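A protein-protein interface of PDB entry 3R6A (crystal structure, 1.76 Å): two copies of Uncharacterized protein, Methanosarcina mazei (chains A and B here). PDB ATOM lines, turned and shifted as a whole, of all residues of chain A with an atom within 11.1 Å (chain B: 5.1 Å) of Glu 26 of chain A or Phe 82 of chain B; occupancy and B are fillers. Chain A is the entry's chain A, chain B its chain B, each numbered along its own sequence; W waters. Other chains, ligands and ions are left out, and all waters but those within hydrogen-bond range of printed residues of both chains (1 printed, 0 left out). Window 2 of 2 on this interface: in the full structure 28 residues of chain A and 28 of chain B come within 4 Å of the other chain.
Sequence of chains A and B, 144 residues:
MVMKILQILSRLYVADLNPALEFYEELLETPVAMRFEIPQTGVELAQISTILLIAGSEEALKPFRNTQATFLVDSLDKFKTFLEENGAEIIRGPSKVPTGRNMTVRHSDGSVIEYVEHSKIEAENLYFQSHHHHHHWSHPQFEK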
ATOM      1  N   LEU A  17     -12.992   5.183   7.107  1.00  0.00           N
ATOM      2  CA  LEU A  17     -13.429   6.509   7.521  1.00  0.00           C
ATOM      3  C   LEU A  17     -12.788   7.065   8.798  1.00  0.00           C
ATOM      4  O   LEU A  17     -12.215   8.153   8.785  1.00  0.00           O
ATOM      5  CB  LEU A  17     -14.952   6.507   7.677  1.00  0.00           C
ATOM      6  CG  LEU A  17     -15.697   7.830   7.502  1.00  0.00           C
ATOM      7  CD1 LEU A  17     -17.190   7.580   7.606  1.00  0.00           C
ATOM      8  CD2 LEU A  17     -15.249   8.831   8.553  1.00  0.00           C
ATOM      9  N   ASN A  18     -12.886   6.316   9.892  1.00  0.00           N
ATOM     10  CA  ASN A  18     -12.372   6.763  11.186  1.00  0.00           C
ATOM     11  C   ASN A  18     -10.980   7.387  11.242  1.00  0.00           C
ATOM     12  O   ASN A  18     -10.831   8.522  11.703  1.00  0.00           O
ATOM     13  CB  ASN A  18     -12.466   5.627  12.206  1.00  0.00           C
ATOM     14  CG  ASN A  18     -13.897   5.202  12.461  1.00  0.00           C
ATOM     15  OD1 ASN A  18     -14.800   6.038  12.513  1.00  0.00           O
ATOM     16  ND2 ASN A  18     -14.112   3.901  12.635  1.00  0.00           N
ATOM     17  N   PRO A  19      -9.940   6.659  10.802  1.00  0.00           N
ATOM     18  CA  PRO A  19      -8.608   7.269  10.860  1.00  0.00           C
ATOM     19  C   PRO A  19      -8.507   8.520   9.988  1.00  0.00           C
ATOM     20  O   PRO A  19      -7.898   9.521  10.377  1.00  0.00           O
ATOM     21  CB  PRO A  19      -7.688   6.137  10.396  1.00  0.00           C
ATOM     22  CG  PRO A  19      -8.565   5.320   9.508  1.00  0.00           C
ATOM     23  CD  PRO A  19      -9.871   5.293  10.254  1.00  0.00           C
ATOM     24  N   ALA A  20      -9.122   8.463   8.814  1.00  0.00           N
ATOM     25  CA  ALA A  20      -9.108   9.592   7.890  1.00  0.00           C
ATOM     26  C   ALA A  20      -9.827  10.793   8.495  1.00  0.00           C
ATOM     27  O   ALA A  20      -9.352  11.921   8.416  1.00  0.00           O
ATOM     28  CB  ALA A  20      -9.768   9.195   6.578  1.00  0.00           C
ATOM     29  N   LEU A  21     -10.978  10.548   9.109  1.00  0.00           N
ATOM     30  CA  LEU A  21     -11.745  11.627   9.706  1.00  0.00           C
ATOM     31  C   LEU A  21     -10.891  12.387  10.722  1.00  0.00           C
ATOM     32  O   LEU A  21     -10.894  13.619  10.754  1.00  0.00           O
ATOM     33  CB  LEU A  21     -13.001  11.055  10.365  1.00  0.00           C
ATOM     34  CG  LEU A  21     -14.219  11.963  10.529  1.00  0.00           C
ATOM     35  CD1 LEU A  21     -14.510  12.707   9.226  1.00  0.00           C
ATOM     36  CD2 LEU A  21     -15.412  11.108  10.942  1.00  0.00           C
ATOM     37  N   GLU A  22     -10.137  11.654  11.533  1.00  0.00           N
ATOM     38  CA  GLU A  22      -9.285  12.285  12.536  1.00  0.00           C
ATOM     39  C   GLU A  22      -8.226  13.155  11.867  1.00  0.00           C
ATOM     40  O   GLU A  22      -7.933  14.257  12.326  1.00  0.00           O
ATOM     41  CB  GLU A  22      -8.612  11.219  13.401  1.00  0.00           C
ATOM     42  CG  GLU A  22      -7.877  11.779  14.612  1.00  0.00           C
ATOM     43  CD  GLU A  22      -8.755  12.676  15.473  1.00  0.00           C
ATOM     44  OE1 GLU A  22      -9.850  12.232  15.892  1.00  0.00           O
ATOM     45  OE2 GLU A  22      -8.345  13.828  15.735  1.00  0.00           O
ATOM     46  N   PHE A  23      -7.664  12.656  10.772  1.00  0.00           N
ATOM     47  CA  PHE A  23      -6.640  13.388  10.041  1.00  0.00           C
ATOM     48  C   PHE A  23      -7.183  14.697   9.472  1.00  0.00           C
ATOM     49  O   PHE A  23      -6.590  15.758   9.665  1.00  0.00           O
ATOM     50  CB  PHE A  23      -6.089  12.522   8.908  1.00  0.00           C
ATOM     51  CG  PHE A  23      -5.176  13.260   7.972  1.00  0.00           C
ATOM     52  CD1 PHE A  23      -3.890  13.615   8.365  1.00  0.00           C
ATOM     53  CD2 PHE A  23      -5.609  13.612   6.698  1.00  0.00           C
ATOM     54  CE1 PHE A  23      -3.045  14.312   7.507  1.00  0.00           C
ATOM     55  CE2 PHE A  23      -4.772  14.312   5.828  1.00  0.00           C
ATOM     56  CZ  PHE A  23      -3.484  14.663   6.233  1.00  0.00           C
ATOM     57  N   TYR A  24      -8.313  14.629   8.774  1.00  0.00           N
ATOM     58  CA  TYR A  24      -8.886  15.838   8.189  1.00  0.00           C
ATOM     59  C   TYR A  24      -9.397  16.835   9.226  1.00  0.00           C
ATOM     60  O   TYR A  24      -9.364  18.035   8.999  1.00  0.00           O
ATOM     61  CB  TYR A  24      -9.983  15.469   7.190  1.00  0.00           C
ATOM     62  CG  TYR A  24      -9.403  14.839   5.946  1.00  0.00           C
ATOM     63  CD1 TYR A  24      -8.671  15.606   5.036  1.00  0.00           C
ATOM     64  CD2 TYR A  24      -9.477  13.465   5.738  1.00  0.00           C
ATOM     65  CE1 TYR A  24      -8.015  15.014   3.957  1.00  0.00           C
ATOM     66  CE2 TYR A  24      -8.821  12.860   4.658  1.00  0.00           C
ATOM     67  CZ  TYR A  24      -8.089  13.644   3.778  1.00  0.00           C
ATOM     68  OH  TYR A  24      -7.388  13.052   2.750  1.00  0.00           O
ATOM     69  N   GLU A  25      -9.867  16.351  10.371  1.00  0.00           N
ATOM     70  CA  GLU A  25     -10.332  17.275  11.400  1.00  0.00           C
ATOM     71  C   GLU A  25      -9.136  18.112  11.859  1.00  0.00           C
ATOM     72  O   GLU A  25      -9.254  19.314  12.087  1.00  0.00           O
ATOM     73  CB  GLU A  25     -10.938  16.503  12.579  1.00  0.00           C
ATOM     74  CG  GLU A  25     -12.216  15.764  12.206  1.00  0.00           C
ATOM     75  CD  GLU A  25     -12.652  14.749  13.247  1.00  0.00           C
ATOM     76  OE1 GLU A  25     -11.794  14.254  14.007  1.00  0.00           O
ATOM     77  OE2 GLU A  25     -13.856  14.429  13.285  1.00  0.00           O
ATOM     78  N   GLU A  26      -7.977  17.475  11.977  1.00  0.00           N
ATOM     79  CA  GLU A  26      -6.769  18.175  12.394  1.00  0.00           C
ATOM     80  C   GLU A  26      -6.253  19.074  11.278  1.00  0.00           C
ATOM     81  O   GLU A  26      -5.922  20.238  11.504  1.00  0.00           O
ATOM     82  CB  GLU A  26      -5.680  17.172  12.774  1.00  0.00           C
ATOM     83  CG  GLU A  26      -5.966  16.398  14.050  1.00  0.00           C
ATOM     84  CD  GLU A  26      -5.027  15.222  14.242  1.00  0.00           C
ATOM     85  OE1 GLU A  26      -3.798  15.409  14.104  1.00  0.00           O
ATOM     86  OE2 GLU A  26      -5.518  14.109  14.535  1.00  0.00           O
ATOM     87  N   LEU A  27      -6.182  18.523  10.071  1.00  0.00           N
ATOM     88  CA  LEU A  27      -5.686  19.267   8.918  1.00  0.00           C
ATOM     89  C   LEU A  27      -6.507  20.512   8.628  1.00  0.00           C
ATOM     90  O   LEU A  27      -5.957  21.566   8.323  1.00  0.00           O
ATOM     91  CB  LEU A  27      -5.679  18.371   7.673  1.00  0.00           C
ATOM     92  CG  LEU A  27      -5.212  19.027   6.369  1.00  0.00           C
ATOM     93  CD1 LEU A  27      -3.728  19.388   6.470  1.00  0.00           C
ATOM     94  CD2 LEU A  27      -5.446  18.070   5.204  1.00  0.00           C
ATOM     95  N   LEU A  28      -7.824  20.384   8.730  1.00  0.00           N
ATOM     96  CA  LEU A  28      -8.723  21.492   8.442  1.00  0.00           C
ATOM     97  C   LEU A  28      -9.135  22.253   9.701  1.00  0.00           C
ATOM     98  O   LEU A  28      -9.964  23.158   9.638  1.00  0.00           O
ATOM     99  CB  LEU A  28      -9.970  20.962   7.719  1.00  0.00           C
ATOM    100  CG  LEU A  28      -9.712  20.001   6.546  1.00  0.00           C
ATOM    101  CD1 LEU A  28     -11.021  19.400   6.068  1.00  0.00           C
ATOM    102  CD2 LEU A  28      -9.019  20.730   5.411  1.00  0.00           C
ATOM    103  N   GLU A  29      -8.544  21.888  10.837  1.00  0.00           N
ATOM    104  CA  GLU A  29      -8.863  22.525  12.113  1.00  0.00           C
ATOM    105  C   GLU A  29     -10.374  22.645  12.301  1.00  0.00           C
ATOM    106  O   GLU A  29     -10.893  23.689  12.693  1.00  0.00           O
ATOM    107  CB  GLU A  29      -8.195  23.903  12.200  1.00  0.00           C
ATOM    108  CG  GLU A  29      -6.699  23.822  12.478  1.00  0.00           C
ATOM    109  CD  GLU A  29      -6.022  25.179  12.481  1.00  0.00           C
ATOM    110  OE1 GLU A  29      -6.641  26.153  12.967  1.00  0.00           O
ATOM    111  OE2 GLU A  29      -4.867  25.271  12.013  1.00  0.00           O
ATOM    112  N   THR A  30     -11.068  21.551  12.002  1.00  0.00           N
ATOM    113  CA  THR A  30     -12.518  21.467  12.122  1.00  0.00           C
ATOM    114  C   THR A  30     -12.768  20.231  12.986  1.00  0.00           C
ATOM    115  O   THR A  30     -12.682  19.097  12.507  1.00  0.00           O
ATOM    116  CB  THR A  30     -13.158  21.294  10.735  1.00  0.00           C
ATOM    117  OG1 THR A  30     -12.742  22.375   9.888  1.00  0.00           O
ATOM    118  CG2 THR A  30     -14.673  21.297  10.834  1.00  0.00           C
ATOM    119  N   PRO A  31     -13.087  20.438  14.276  1.00  0.00           N
ATOM    120  CA  PRO A  31     -13.334  19.342  15.220  1.00  0.00           C
ATOM    121  C   PRO A  31     -14.668  18.607  15.154  1.00  0.00           C
ATOM    122  O   PRO A  31     -14.939  17.737  15.987  1.00  0.00           O
ATOM    123  CB  PRO A  31     -13.117  20.015  16.571  1.00  0.00           C
ATOM    124  CG  PRO A  31     -13.715  21.370  16.342  1.00  0.00           C
ATOM    125  CD  PRO A  31     -13.221  21.747  14.942  1.00  0.00           C
ATOM    126  N   VAL A  32     -15.496  18.941  14.174  1.00  0.00           N
ATOM    127  CA  VAL A  32     -16.796  18.292  14.029  1.00  0.00           C
ATOM    128  C   VAL A  32     -17.047  17.919  12.573  1.00  0.00           C
ATOM    129  O   VAL A  32     -16.747  18.694  11.670  1.00  0.00           O
ATOM    130  CB  VAL A  32     -17.930  19.223  14.507  1.00  0.00           C
ATOM    131  CG1 VAL A  32     -19.286  18.558  14.284  1.00  0.00           C
ATOM    132  CG2 VAL A  32     -17.736  19.552  15.980  1.00  0.00           C
ATOM    133  N   ALA A  33     -17.579  16.721  12.361  1.00  0.00           N
ATOM    134  CA  ALA A  33     -17.895  16.223  11.024  1.00  0.00           C
ATOM    135  C   ALA A  33     -19.303  15.653  11.065  1.00  0.00           C
ATOM    136  O   ALA A  33     -19.830  15.348  12.134  1.00  0.00           O
ATOM    137  CB  ALA A  33     -16.913  15.133  10.614  1.00  0.00           C
ATOM    138  N   ILE A  48     -16.701  16.885   6.155  1.00  0.00           N
ATOM    139  CA  ILE A  48     -15.852  17.657   7.053  1.00  0.00           C
ATOM    140  C   ILE A  48     -15.570  18.923   6.263  1.00  0.00           C
ATOM    141  O   ILE A  48     -15.021  18.857   5.168  1.00  0.00           O
ATOM    142  CB  ILE A  48     -14.539  16.907   7.402  1.00  0.00           C
ATOM    143  CG1 ILE A  48     -13.689  17.765   8.338  1.00  0.00           C
ATOM    144  CG2 ILE A  48     -13.776  16.530   6.146  1.00  0.00           C
ATOM    145  CD1 ILE A  48     -14.359  18.061   9.656  1.00  0.00           C
ATOM    146  N   SER A  49     -15.966  20.068   6.809  1.00  0.00           N
ATOM    147  CA  SER A  49     -15.812  21.342   6.107  1.00  0.00           C
ATOM    148  C   SER A  49     -16.572  21.138   4.787  1.00  0.00           C
ATOM    149  O   SER A  49     -17.710  20.665   4.810  1.00  0.00           O
ATOM    150  CB  SER A  49     -14.333  21.656   5.849  1.00  0.00           C
ATOM    151  OG  SER A  49     -14.185  22.950   5.287  1.00  0.00           O
ATOM    152  N   ILE A  51     -15.607  19.090   2.370  1.00  0.00           N
ATOM    153  CA  ILE A  51     -15.085  17.851   1.804  1.00  0.00           C
ATOM    154  C   ILE A  51     -16.007  16.698   2.165  1.00  0.00           C
ATOM    155  O   ILE A  51     -16.459  16.587   3.311  1.00  0.00           O
ATOM    156  CB  ILE A  51     -13.685  17.496   2.369  1.00  0.00           C
ATOM    157  CG1 ILE A  51     -12.628  18.434   1.784  1.00  0.00           C
ATOM    158  CG2 ILE A  51     -13.340  16.038   2.047  1.00  0.00           C
ATOM    159  CD1 ILE A  51     -11.271  18.296   2.425  1.00  0.00           C
ATOM    160  N   LEU A  53     -16.056  12.760   2.491  1.00  0.00           N
ATOM    161  CA  LEU A  53     -15.163  11.608   2.571  1.00  0.00           C
ATOM    162  C   LEU A  53     -16.022  10.383   2.319  1.00  0.00           C
ATOM    163  O   LEU A  53     -16.981  10.133   3.042  1.00  0.00           O
ATOM    164  CB  LEU A  53     -14.521  11.488   3.956  1.00  0.00           C
ATOM    165  CG  LEU A  53     -13.496  12.521   4.419  1.00  0.00           C
ATOM    166  CD1 LEU A  53     -13.100  12.206   5.856  1.00  0.00           C
ATOM    167  CD2 LEU A  53     -12.268  12.497   3.519  1.00  0.00           C
ATOM    168  N   MET B   3      -1.576  28.204  10.496  1.00  0.00           N
ATOM    169  CA  MET B   3      -1.974  27.199   9.463  1.00  0.00           C
ATOM    170  C   MET B   3      -3.471  27.337   9.192  1.00  0.00           C
ATOM    171  O   MET B   3      -4.294  27.016  10.047  1.00  0.00           O
ATOM    172  CB  MET B   3      -1.655  25.790   9.967  1.00  0.00           C
ATOM    173  CG  MET B   3      -1.773  24.699   8.924  1.00  0.00           C
ATOM    174  SD  MET B   3      -1.166  22.984   9.569  1.00  0.00           S
ATOM    175  CE  MET B   3      -2.870  22.226  10.077  1.00  0.00           C
ATOM    176  N   LYS B  78       3.853  25.832   6.737  1.00  0.00           N
ATOM    177  CA  LYS B  78       3.193  25.318   7.932  1.00  0.00           C
ATOM    178  C   LYS B  78       2.519  23.980   7.640  1.00  0.00           C
ATOM    179  O   LYS B  78       2.605  23.038   8.433  1.00  0.00           O
ATOM    180  CB  LYS B  78       2.157  26.324   8.439  1.00  0.00           C
ATOM    181  CG  LYS B  78       2.520  26.971   9.774  1.00  0.00           C
ATOM    182  CD  LYS B  78       3.850  27.702   9.711  1.00  0.00           C
ATOM    183  CE  LYS B  78       3.776  28.948   8.839  1.00  0.00           C
ATOM    184  NZ  LYS B  78       5.082  29.672   8.794  1.00  0.00           N
ATOM    185  N   PHE B  79       1.851  23.898   6.493  1.00  0.00           N
ATOM    186  CA  PHE B  79       1.170  22.669   6.096  1.00  0.00           C
ATOM    187  C   PHE B  79       2.161  21.566   5.748  1.00  0.00           C
ATOM    188  O   PHE B  79       1.932  20.401   6.053  1.00  0.00           O
ATOM    189  CB  PHE B  79       0.242  22.936   4.904  1.00  0.00           C
ATOM    190  CG  PHE B  79      -1.094  23.497   5.298  1.00  0.00           C
ATOM    191  CD1 PHE B  79      -2.114  22.654   5.725  1.00  0.00           C
ATOM    192  CD2 PHE B  79      -1.319  24.871   5.289  1.00  0.00           C
ATOM    193  CE1 PHE B  79      -3.342  23.166   6.142  1.00  0.00           C
ATOM    194  CE2 PHE B  79      -2.545  25.396   5.704  1.00  0.00           C
ATOM    195  CZ  PHE B  79      -3.557  24.542   6.132  1.00  0.00           C
ATOM    196  N   LYS B  80       3.267  21.938   5.113  1.00  0.00           N
ATOM    197  CA  LYS B  80       4.281  20.962   4.740  1.00  0.00           C
ATOM    198  C   LYS B  80       4.768  20.230   5.985  1.00  0.00           C
ATOM    199  O   LYS B  80       4.867  19.004   5.996  1.00  0.00           O
ATOM    200  CB  LYS B  80       5.455  21.658   4.045  1.00  0.00           C
ATOM    201  CG  LYS B  80       6.537  20.719   3.538  1.00  0.00           C
ATOM    202  CD  LYS B  80       7.573  21.488   2.725  1.00  0.00           C
ATOM    203  CE  LYS B  80       8.675  20.574   2.210  1.00  0.00           C
ATOM    204  NZ  LYS B  80       9.479  19.991   3.317  1.00  0.00           N
ATOM    205  N   THR B  81       5.059  20.993   7.033  1.00  0.00           N
ATOM    206  CA  THR B  81       5.533  20.427   8.288  1.00  0.00           C
ATOM    207  C   THR B  81       4.493  19.479   8.876  1.00  0.00           C
ATOM    208  O   THR B  81       4.795  18.333   9.192  1.00  0.00           O
ATOM    209  CB  THR B  81       5.843  21.537   9.309  1.00  0.00           C
ATOM    210  OG1 THR B  81       6.834  22.417   8.764  1.00  0.00           O
ATOM    211  CG2 THR B  81       6.365  20.936  10.618  1.00  0.00           C
ATOM    212  N   PHE B  82       3.262  19.961   9.012  1.00  0.00           N
ATOM    213  CA  PHE B  82       2.182  19.145   9.556  1.00  0.00           C
ATOM    214  C   PHE B  82       2.024  17.859   8.756  1.00  0.00           C
ATOM    215  O   PHE B  82       1.954  16.767   9.318  1.00  0.00           O
ATOM    216  CB  PHE B  82       0.857  19.916   9.522  1.00  0.00           C
ATOM    217  CG  PHE B  82      -0.331  19.098   9.948  1.00  0.00           C
ATOM    218  CD1 PHE B  82      -0.632  18.931  11.295  1.00  0.00           C
ATOM    219  CD2 PHE B  82      -1.129  18.462   8.999  1.00  0.00           C
ATOM    220  CE1 PHE B  82      -1.712  18.141  11.695  1.00  0.00           C
ATOM    221  CE2 PHE B  82      -2.210  17.669   9.386  1.00  0.00           C
ATOM    222  CZ  PHE B  82      -2.503  17.509  10.737  1.00  0.00           C
ATOM    223  N   LEU B  83       1.968  17.994   7.436  1.00  0.00           N
ATOM    224  CA  LEU B  83       1.785  16.838   6.570  1.00  0.00           C
ATOM    225  C   LEU B  83       2.894  15.795   6.704  1.00  0.00           C
ATOM    226  O   LEU B  83       2.617  14.601   6.810  1.00  0.00           O
ATOM    227  CB  LEU B  83       1.646  17.307   5.120  1.00  0.00           C
ATOM    228  CG  LEU B  83       0.332  18.055   4.845  1.00  0.00           C
ATOM    229  CD1 LEU B  83       0.433  18.842   3.545  1.00  0.00           C
ATOM    230  CD2 LEU B  83      -0.818  17.052   4.768  1.00  0.00           C
ATOM    231  N   GLU B  84       4.144  16.244   6.714  1.00  0.00           N
ATOM    232  CA  GLU B  84       5.268  15.320   6.834  1.00  0.00           C
ATOM    233  C   GLU B  84       5.267  14.602   8.181  1.00  0.00           C
ATOM    234  O   GLU B  84       5.750  13.475   8.290  1.00  0.00           O
ATOM    235  CB  GLU B  84       6.591  16.070   6.657  1.00  0.00           C
ATOM    236  CG  GLU B  84       6.729  16.770   5.319  1.00  0.00           C
ATOM    237  CD  GLU B  84       8.042  17.515   5.189  1.00  0.00           C
ATOM    238  OE1 GLU B  84       8.391  18.266   6.125  1.00  0.00           O
ATOM    239  OE2 GLU B  84       8.719  17.358   4.153  1.00  0.00           O
ATOM    240  N   GLU B  85       4.729  15.257   9.203  1.00  0.00           N
ATOM    241  CA  GLU B  85       4.674  14.670  10.539  1.00  0.00           C
ATOM    242  C   GLU B  85       3.410  13.842  10.717  1.00  0.00           C
ATOM    243  O   GLU B  85       3.179  13.266  11.782  1.00  0.00           O
ATOM    244  CB  GLU B  85       4.711  15.772  11.602  1.00  0.00           C
ATOM    245  CG  GLU B  85       5.833  16.776  11.403  1.00  0.00           C
ATOM    246  CD  GLU B  85       5.888  17.823  12.496  1.00  0.00           C
ATOM    247  OE1 GLU B  85       4.818  18.336  12.890  1.00  0.00           O
ATOM    248  OE2 GLU B  85       7.007  18.144  12.954  1.00  0.00           O
ATOM    249  N   ASN B  86       2.589  13.776   9.675  1.00  0.00           N
ATOM    250  CA  ASN B  86       1.351  13.017   9.766  1.00  0.00           C
ATOM    251  C   ASN B  86       1.121  12.000   8.652  1.00  0.00           C
ATOM    252  O   ASN B  86      -0.001  11.831   8.172  1.00  0.00           O
ATOM    253  CB  ASN B  86       0.172  13.985   9.876  1.00  0.00           C
ATOM    254  CG  ASN B  86       0.056  14.598  11.263  1.00  0.00           C
ATOM    255  OD1 ASN B  86      -0.448  13.966  12.193  1.00  0.00           O
ATOM    256  ND2 ASN B  86       0.540  15.824  11.414  1.00  0.00           N
HETATM  257  O   HOH W   1      -2.765  27.452  13.469  1.00  0.00           O
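The side-chain carboxylate (OE2) of Glu 29 of chain A sits close to the backbone carbonyl oxygen (O) of Met 3 of chain B (2.7 Å).
Hydrophobic or aromatic side chains of chain B that line the printed part of chain A: Met 3, Phe 79, Phe 82 and Leu 83. Of the 21 printed residues of chain A, 4 touch a printed residue of chain B. Hydrophobic or aromatic side chains of chain A that line the printed part of chain B: Phe 23 and Leu 27. Among the printed residues, 9 pairs touch across the chains. Among the printed residues, no Asp or Glu carboxylate lies within 4 Å of a Lys or Arg side-chain nitrogen of the other chain.
Of chain B, only Met 3 and Phe 82 come within 4 Å of Glu 26 of chain A. Phe 82 of chain B touches three residues of chain A. No residue of chain A comes within 4 Å of Thr 81 of chain B. Of the printed residues of chain A, Leu 83 of chain B touches Phe 23 (3.9 Å). Glu 85 of chain B touches none of the printed residues of chain A. Of the printed residues of chain A, Phe 79 of chain B touches Leu 27. Of the printed residues of chain A, Met 3 of chain B touches Glu 26, Leu 27 and Glu 29. The nearest residue of chain B that does not touch Glu 26 of chain A is Asn 86 of chain B (4.1 Å). The nearest residue of chain A that does not touch Phe 82 of chain B is Leu 28 of chain A (6.3 Å). The nearest printed residue of chain B that does not touch Glu 29 of chain A is Phe 79 of chain B (6.1 Å).
Phe 82 of chain B touches Phe 23 of chain A. Leu 83 of chain B touches Phe 23 of chain A. Asn 86 of chain B touches Phe 23 of chain A. Met 3 of chain B touches Glu 26 of chain A (CE to O, 3.9 Å). Glu 26 of chain A touches Phe 82 of chain B (CB to CZ, 3.8 Å). Met 3 of chain B touches Leu 27 of chain A (CE to O, 3.6 Å). Leu 27 of chain A touches Phe 79 of chain B (CD1 to CD1, 3.7 Å). Leu 27 of chain A touches Phe 82 of chain B (CD1 to CE2, 3.7 Å).
No position is printed for both chains. Of the 9 pairs that touch across the chains among the printed residues, none has its exchanged pair printed and touching as well.
O of Phe 82 of chain B lies within hydrogen-bond range of ND2 of Asn 86 of chain B (2.7 Å).
Water W1 lies within hydrogen-bond range of N of Met 3 of chain B (3.3 Å) and OE2 of Glu 29 of chain A (3.4 Å).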
